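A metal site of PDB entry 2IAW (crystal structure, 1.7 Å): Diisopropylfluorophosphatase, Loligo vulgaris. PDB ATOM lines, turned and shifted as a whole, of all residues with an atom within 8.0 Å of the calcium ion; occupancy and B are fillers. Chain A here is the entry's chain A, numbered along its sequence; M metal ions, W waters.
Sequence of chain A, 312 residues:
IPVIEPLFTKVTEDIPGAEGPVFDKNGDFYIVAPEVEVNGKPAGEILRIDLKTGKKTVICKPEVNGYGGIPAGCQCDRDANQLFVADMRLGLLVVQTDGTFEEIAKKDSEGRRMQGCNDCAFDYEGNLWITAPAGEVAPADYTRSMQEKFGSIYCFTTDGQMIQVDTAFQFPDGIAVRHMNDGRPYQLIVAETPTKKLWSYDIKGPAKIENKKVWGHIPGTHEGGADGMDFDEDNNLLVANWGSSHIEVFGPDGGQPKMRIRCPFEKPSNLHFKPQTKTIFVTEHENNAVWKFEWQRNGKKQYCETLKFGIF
The side-chain amide oxygen of Gln 302 sits close to the side-chain carboxylate of Asp 230, at 3.4 Å. O of Asp 230 is in hydrogen-bond range of N of Leu 238, at 2.8 Å. A ring nitrogen (ND1) of His 272 sits close to the backbone carbonyl oxygen of Pro 21 (3.3 Å). The backbone NH of Phe 281 is in hydrogen-bond range of the backbone carbonyl oxygen of His 272, at 2.9 Å. The side-chain amide oxygen (OD1) of Asn 270 lies close to the side-chain carboxylate (OD2) of Asp 119, at 3.0 Å. The side-chain amide oxygen (OD1) of Asn 270 sits close to the side-chain carboxylate (OE1) of Glu 19.
ND2 of Asn 270 touches the calcium ion, 3.97 Å away. Four residues have an atom within 4 Å of the calcium ion: Asp 230, Asn 270, Leu 271 and His 272. The nearest printed residue that does not touch the calcium ion is Pro 21 (4.1 Å).
The calcium ion is bound by OD2 of Asp 230, at 2.2 Å. Water W3 is bound to the calcium ion (2.2 Å). Water W2 is bound to the calcium ion, at 2.3 Å. The calcium ion is bound by O of Leu 271, at 2.3 Å. The calcium ion is bound by water W1 (2.3 Å). The calcium ion is bound by a ring nitrogen (ND1) of His 272.
Water W3 lies within hydrogen-bond range of ND2 of Asn 270 and O of Met 229. Water W1 lies within hydrogen-bond range of the side-chain carboxylate of Asp 230 (2.8 Å) and the side-chain amide oxygen of Gln 75 (3.2 Å).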
ATOM      1  N   GLU A  19      15.300  16.594 -22.975  1.00  0.00           N
ATOM      2  CA  GLU A  19      16.712  16.282 -23.257  1.00  0.00           C
ATOM      3  C   GLU A  19      17.615  17.150 -22.402  1.00  0.00           C
ATOM      4  O   GLU A  19      17.136  17.962 -21.616  1.00  0.00           O
ATOM      5  CB  GLU A  19      16.991  16.651 -24.727  1.00  0.00           C
ATOM      6  CG  GLU A  19      17.165  15.455 -25.667  1.00  0.00           C
ATOM      7  CD  GLU A  19      18.567  14.847 -25.617  1.00  0.00           C
ATOM      8  OE1 GLU A  19      19.264  15.056 -24.600  1.00  0.00           O
ATOM      9  OE2 GLU A  19      18.951  14.133 -26.579  1.00  0.00           O
ATOM     10  N   GLY A  20      18.938  16.970 -22.543  1.00  0.00           N
ATOM     11  CA  GLY A  20      19.911  17.845 -21.889  1.00  0.00           C
ATOM     12  C   GLY A  20      19.783  18.158 -20.418  1.00  0.00           C
ATOM     13  O   GLY A  20      19.945  19.330 -20.023  1.00  0.00           O
ATOM     14  N   PRO A  21      19.554  17.165 -19.570  1.00  0.00           N
ATOM     15  CA  PRO A  21      19.463  17.441 -18.127  1.00  0.00           C
ATOM     16  C   PRO A  21      20.800  17.913 -17.603  1.00  0.00           C
ATOM     17  O   PRO A  21      21.844  17.375 -18.047  1.00  0.00           O
ATOM     18  CB  PRO A  21      19.153  16.088 -17.521  1.00  0.00           C
ATOM     19  CG  PRO A  21      19.661  15.063 -18.510  1.00  0.00           C
ATOM     20  CD  PRO A  21      19.426  15.708 -19.882  1.00  0.00           C
ATOM     21  N   VAL A  22      20.799  18.929 -16.744  1.00  0.00           N
ATOM     22  CA  VAL A  22      22.069  19.447 -16.252  1.00  0.00           C
ATOM     23  C   VAL A  22      21.829  20.180 -14.922  1.00  0.00           C
ATOM     24  O   VAL A  22      20.728  20.684 -14.685  1.00  0.00           O
ATOM     25  CB  VAL A  22      22.664  20.437 -17.293  1.00  0.00           C
ATOM     26  CG1 VAL A  22      21.736  21.648 -17.500  1.00  0.00           C
ATOM     27  CG2 VAL A  22      24.139  20.846 -16.947  1.00  0.00           C
ATOM     28  N   PHE A  23      22.840  20.166 -14.059  1.00  0.00           N
ATOM     29  CA  PHE A  23      22.808  20.909 -12.812  1.00  0.00           C
ATOM     30  C   PHE A  23      23.784  22.069 -12.911  1.00  0.00           C
ATOM     31  O   PHE A  23      24.918  21.907 -13.429  1.00  0.00           O
ATOM     32  CB  PHE A  23      23.191  20.038 -11.601  1.00  0.00           C
ATOM     33  CG  PHE A  23      22.060  19.141 -11.126  1.00  0.00           C
ATOM     34  CD1 PHE A  23      21.112  19.613 -10.243  1.00  0.00           C
ATOM     35  CD2 PHE A  23      21.941  17.857 -11.608  1.00  0.00           C
ATOM     36  CE1 PHE A  23      20.068  18.816  -9.810  1.00  0.00           C
ATOM     37  CE2 PHE A  23      20.872  17.025 -11.198  1.00  0.00           C
ATOM     38  CZ  PHE A  23      19.944  17.493 -10.304  1.00  0.00           C
ATOM     39  N   CYS A  74      23.256  19.975 -22.888  1.00  0.00           N
ATOM     40  CA  CYS A  74      23.815  21.031 -22.068  1.00  0.00           C
ATOM     41  C   CYS A  74      25.044  20.624 -21.250  1.00  0.00           C
ATOM     42  O   CYS A  74      25.189  19.447 -20.843  1.00  0.00           O
ATOM     43  CB  CYS A  74      22.776  21.386 -21.034  1.00  0.00           C
ATOM     44  SG  CYS A  74      21.205  21.995 -21.692  1.00  0.00           S
ATOM     45  N   GLN A  75      25.866  21.604 -20.904  1.00  0.00           N
ATOM     46  CA  GLN A  75      26.898  21.368 -19.919  1.00  0.00           C
ATOM     47  C   GLN A  75      26.957  22.657 -19.134  1.00  0.00           C
ATOM     48  O   GLN A  75      26.737  23.712 -19.707  1.00  0.00           O
ATOM     49  CB  GLN A  75      28.262  21.235 -20.630  1.00  0.00           C
ATOM     50  CG  GLN A  75      28.541  19.875 -21.245  1.00  0.00           C
ATOM     51  CD  GLN A  75      28.703  18.785 -20.231  1.00  0.00           C
ATOM     52  OE1 GLN A  75      27.703  18.166 -19.789  1.00  0.00           O
ATOM     53  NE2 GLN A  75      29.924  18.505 -19.870  1.00  0.00           N
ATOM     54  N   ASP A 119      24.849  17.355 -28.490  1.00  0.00           N
ATOM     55  CA  ASP A 119      25.264  17.192 -27.078  1.00  0.00           C
ATOM     56  C   ASP A 119      26.714  17.629 -26.932  1.00  0.00           C
ATOM     57  O   ASP A 119      27.428  17.874 -27.927  1.00  0.00           O
ATOM     58  CB  ASP A 119      25.041  15.735 -26.618  1.00  0.00           C
ATOM     59  CG  ASP A 119      24.698  15.631 -25.125  1.00  0.00           C
ATOM     60  OD1 ASP A 119      24.811  16.636 -24.422  1.00  0.00           O
ATOM     61  OD2 ASP A 119      24.304  14.580 -24.601  1.00  0.00           O
ATOM     62  N   CYS A 120      27.139  17.841 -25.686  1.00  0.00           N
ATOM     63  CA  CYS A 120      28.516  18.327 -25.508  1.00  0.00           C
ATOM     64  C   CYS A 120      29.027  17.871 -24.174  1.00  0.00           C
ATOM     65  O   CYS A 120      28.268  17.459 -23.292  1.00  0.00           O
ATOM     66  CB  CYS A 120      28.650  19.857 -25.681  1.00  0.00           C
ATOM     67  SG  CYS A 120      27.528  20.826 -24.595  1.00  0.00           S
ATOM     68  N   ILE A 175      28.128  12.227 -26.002  1.00  0.00           N
ATOM     69  CA  ILE A 175      29.571  12.352 -26.027  1.00  0.00           C
ATOM     70  C   ILE A 175      30.013  12.450 -24.581  1.00  0.00           C
ATOM     71  O   ILE A 175      29.268  12.945 -23.705  1.00  0.00           O
ATOM     72  CB  ILE A 175      29.956  13.602 -26.882  1.00  0.00           C
ATOM     73  CG1 ILE A 175      31.486  13.774 -27.005  1.00  0.00           C
ATOM     74  CG2 ILE A 175      29.193  14.887 -26.339  1.00  0.00           C
ATOM     75  CD1 ILE A 175      31.879  14.715 -28.148  1.00  0.00           C
ATOM     76  N   GLY A 228      22.142   9.980 -24.977  1.00  0.00           N
ATOM     77  CA  GLY A 228      23.082  10.634 -24.046  1.00  0.00           C
ATOM     78  C   GLY A 228      23.882   9.667 -23.170  1.00  0.00           C
ATOM     79  O   GLY A 228      23.514   8.518 -22.977  1.00  0.00           O
ATOM     80  N   MET A 229      24.989  10.153 -22.620  1.00  0.00           N
ATOM     81  CA  MET A 229      25.848   9.324 -21.768  1.00  0.00           C
ATOM     82  C   MET A 229      26.553  10.146 -20.716  1.00  0.00           C
ATOM     83  O   MET A 229      26.674  11.364 -20.854  1.00  0.00           O
ATOM     84  CB  MET A 229      26.951   8.660 -22.627  1.00  0.00           C
ATOM     85  CG  MET A 229      27.810   9.678 -23.350  1.00  0.00           C
ATOM     86  SD  MET A 229      29.113   8.924 -24.372  1.00  0.00           S
ATOM     87  CE  MET A 229      28.009   8.026 -25.420  1.00  0.00           C
ATOM     88  N   ASP A 230      27.063   9.445 -19.706  1.00  0.00           N
ATOM     89  CA  ASP A 230      27.891  10.086 -18.674  1.00  0.00           C
ATOM     90  C   ASP A 230      28.616   8.995 -17.935  1.00  0.00           C
ATOM     91  O   ASP A 230      28.170   7.832 -17.861  1.00  0.00           O
ATOM     92  CB  ASP A 230      27.057  10.843 -17.619  1.00  0.00           C
ATOM     93  CG  ASP A 230      26.880  12.334 -17.946  1.00  0.00           C
ATOM     94  OD1 ASP A 230      27.854  13.033 -18.370  1.00  0.00           O
ATOM     95  OD2 ASP A 230      25.777  12.869 -17.773  1.00  0.00           O
ATOM     96  N   PHE A 231      29.741   9.390 -17.337  1.00  0.00           N
ATOM     97  CA  PHE A 231      30.520   8.472 -16.540  1.00  0.00           C
ATOM     98  C   PHE A 231      30.136   8.512 -15.072  1.00  0.00           C
ATOM     99  O   PHE A 231      29.766   9.568 -14.502  1.00  0.00           O
ATOM    100  CB  PHE A 231      31.988   8.857 -16.613  1.00  0.00           C
ATOM    101  CG  PHE A 231      32.670   8.425 -17.874  1.00  0.00           C
ATOM    102  CD1 PHE A 231      32.969   7.071 -18.094  1.00  0.00           C
ATOM    103  CD2 PHE A 231      33.060   9.361 -18.796  1.00  0.00           C
ATOM    104  CE1 PHE A 231      33.641   6.692 -19.257  1.00  0.00           C
ATOM    105  CE2 PHE A 231      33.713   8.995 -19.959  1.00  0.00           C
ATOM    106  CZ  PHE A 231      33.991   7.650 -20.202  1.00  0.00           C
ATOM    107  N   LEU A 238      27.543   5.210 -18.579  1.00  0.00           N
ATOM    108  CA  LEU A 238      26.141   4.869 -18.654  1.00  0.00           C
ATOM    109  C   LEU A 238      25.595   5.543 -19.881  1.00  0.00           C
ATOM    110  O   LEU A 238      25.822   6.734 -20.102  1.00  0.00           O
ATOM    111  CB  LEU A 238      25.382   5.362 -17.418  1.00  0.00           C
ATOM    112  CG  LEU A 238      25.621   4.480 -16.162  1.00  0.00           C
ATOM    113  CD1 LEU A 238      26.987   4.819 -15.546  1.00  0.00           C
ATOM    114  CD2 LEU A 238      24.524   4.660 -15.110  1.00  0.00           C
ATOM    115  N   ASN A 270      18.439  10.904 -22.302  1.00  0.00           N
ATOM    116  CA  ASN A 270      19.668  11.462 -21.764  1.00  0.00           C
ATOM    117  C   ASN A 270      19.668  11.354 -20.255  1.00  0.00           C
ATOM    118  O   ASN A 270      18.663  10.970 -19.666  1.00  0.00           O
ATOM    119  CB  ASN A 270      19.852  12.928 -22.245  1.00  0.00           C
ATOM    120  CG  ASN A 270      21.317  13.328 -22.435  1.00  0.00           C
ATOM    121  OD1 ASN A 270      21.650  14.182 -23.307  1.00  0.00           O
ATOM    122  ND2 ASN A 270      22.210  12.749 -21.652  1.00  0.00           N
ATOM    123  N   LEU A 271      20.795  11.635 -19.614  1.00  0.00           N
ATOM    124  CA  LEU A 271      20.834  11.468 -18.171  1.00  0.00           C
ATOM    125  C   LEU A 271      21.881  12.375 -17.527  1.00  0.00           C
ATOM    126  O   LEU A 271      22.759  12.872 -18.235  1.00  0.00           O
ATOM    127  CB  LEU A 271      21.119   9.996 -17.828  1.00  0.00           C
ATOM    128  CG  LEU A 271      22.327   9.364 -18.512  1.00  0.00           C
ATOM    129  CD1 LEU A 271      23.517   9.691 -17.760  1.00  0.00           C
ATOM    130  CD2 LEU A 271      22.140   7.828 -18.514  1.00  0.00           C
ATOM    131  N   HIS A 272      21.806  12.594 -16.215  1.00  0.00           N
ATOM    132  CA  HIS A 272      22.785  13.436 -15.544  1.00  0.00           C
ATOM    133  C   HIS A 272      22.752  13.112 -14.059  1.00  0.00           C
ATOM    134  O   HIS A 272      21.692  12.998 -13.501  1.00  0.00           O
ATOM    135  CB  HIS A 272      22.425  14.895 -15.679  1.00  0.00           C
ATOM    136  CG  HIS A 272      23.613  15.796 -15.751  1.00  0.00           C
ATOM    137  ND1 HIS A 272      24.440  15.810 -16.842  1.00  0.00           N
ATOM    138  CD2 HIS A 272      24.117  16.720 -14.885  1.00  0.00           C
ATOM    139  CE1 HIS A 272      25.380  16.732 -16.685  1.00  0.00           C
ATOM    140  NE2 HIS A 272      25.220  17.282 -15.489  1.00  0.00           N
ATOM    141  N   PHE A 273      23.911  12.975 -13.429  1.00  0.00           N
ATOM    142  CA  PHE A 273      23.963  12.756 -11.999  1.00  0.00           C
ATOM    143  C   PHE A 273      23.728  14.084 -11.304  1.00  0.00           C
ATOM    144  O   PHE A 273      24.099  15.140 -11.822  1.00  0.00           O
ATOM    145  CB  PHE A 273      25.377  12.293 -11.625  1.00  0.00           C
ATOM    146  CG  PHE A 273      25.626  10.846 -11.899  1.00  0.00           C
ATOM    147  CD1 PHE A 273      26.069  10.426 -13.140  1.00  0.00           C
ATOM    148  CD2 PHE A 273      25.389   9.898 -10.911  1.00  0.00           C
ATOM    149  CE1 PHE A 273      26.318   9.049 -13.389  1.00  0.00           C
ATOM    150  CE2 PHE A 273      25.636   8.532 -11.132  1.00  0.00           C
ATOM    151  CZ  PHE A 273      26.095   8.105 -12.387  1.00  0.00           C
ATOM    152  N   ILE A 280      20.487   9.630 -10.538  1.00  0.00           N
ATOM    153  CA  ILE A 280      20.638   9.980 -11.975  1.00  0.00           C
ATOM    154  C   ILE A 280      19.258  10.440 -12.425  1.00  0.00           C
ATOM    155  O   ILE A 280      18.272   9.742 -12.234  1.00  0.00           O
ATOM    156  CB  ILE A 280      21.064   8.724 -12.764  1.00  0.00           C
ATOM    157  CG1 ILE A 280      22.474   8.337 -12.362  1.00  0.00           C
ATOM    158  CG2 ILE A 280      20.980   8.985 -14.302  1.00  0.00           C
ATOM    159  CD1 ILE A 280      22.991   7.023 -13.112  1.00  0.00           C
ATOM    160  N   PHE A 281      19.224  11.627 -13.032  1.00  0.00           N
ATOM    161  CA  PHE A 281      17.999  12.163 -13.614  1.00  0.00           C
ATOM    162  C   PHE A 281      17.988  11.775 -15.070  1.00  0.00           C
ATOM    163  O   PHE A 281      18.996  11.898 -15.752  1.00  0.00           O
ATOM    164  CB  PHE A 281      18.017  13.688 -13.470  1.00  0.00           C
ATOM    165  CG  PHE A 281      17.756  14.120 -12.083  1.00  0.00           C
ATOM    166  CD1 PHE A 281      18.693  13.942 -11.090  1.00  0.00           C
ATOM    167  CD2 PHE A 281      16.505  14.641 -11.758  1.00  0.00           C
ATOM    168  CE1 PHE A 281      18.416  14.308  -9.785  1.00  0.00           C
ATOM    169  CE2 PHE A 281      16.219  14.994 -10.441  1.00  0.00           C
ATOM    170  CZ  PHE A 281      17.172  14.833  -9.483  1.00  0.00           C
ATOM    171  N   GLN A 302      31.499  16.526 -12.973  1.00  0.00           N
ATOM    172  CA  GLN A 302      31.551  17.330 -14.199  1.00  0.00           C
ATOM    173  C   GLN A 302      32.573  18.438 -14.044  1.00  0.00           C
ATOM    174  O   GLN A 302      32.973  18.783 -12.937  1.00  0.00           O
ATOM    175  CB  GLN A 302      30.162  17.919 -14.487  1.00  0.00           C
ATOM    176  CG  GLN A 302      29.128  16.856 -14.830  1.00  0.00           C
ATOM    177  CD  GLN A 302      29.075  16.589 -16.319  1.00  0.00           C
ATOM    178  OE1 GLN A 302      29.588  15.545 -16.804  1.00  0.00           O
ATOM    179  NE2 GLN A 302      28.539  17.529 -17.063  1.00  0.00           N
HETATM  180 CA    CA M   1      24.502  14.301 -18.812  1.00  0.00          CA
HETATM  181  O   HOH W   1      26.542  15.196 -19.491  1.00  0.00           O
HETATM  182  O   HOH W   2      23.087  15.871 -19.690  1.00  0.00           O
HETATM  183  O   HOH W   3      24.657  13.287 -20.790  1.00  0.00           O
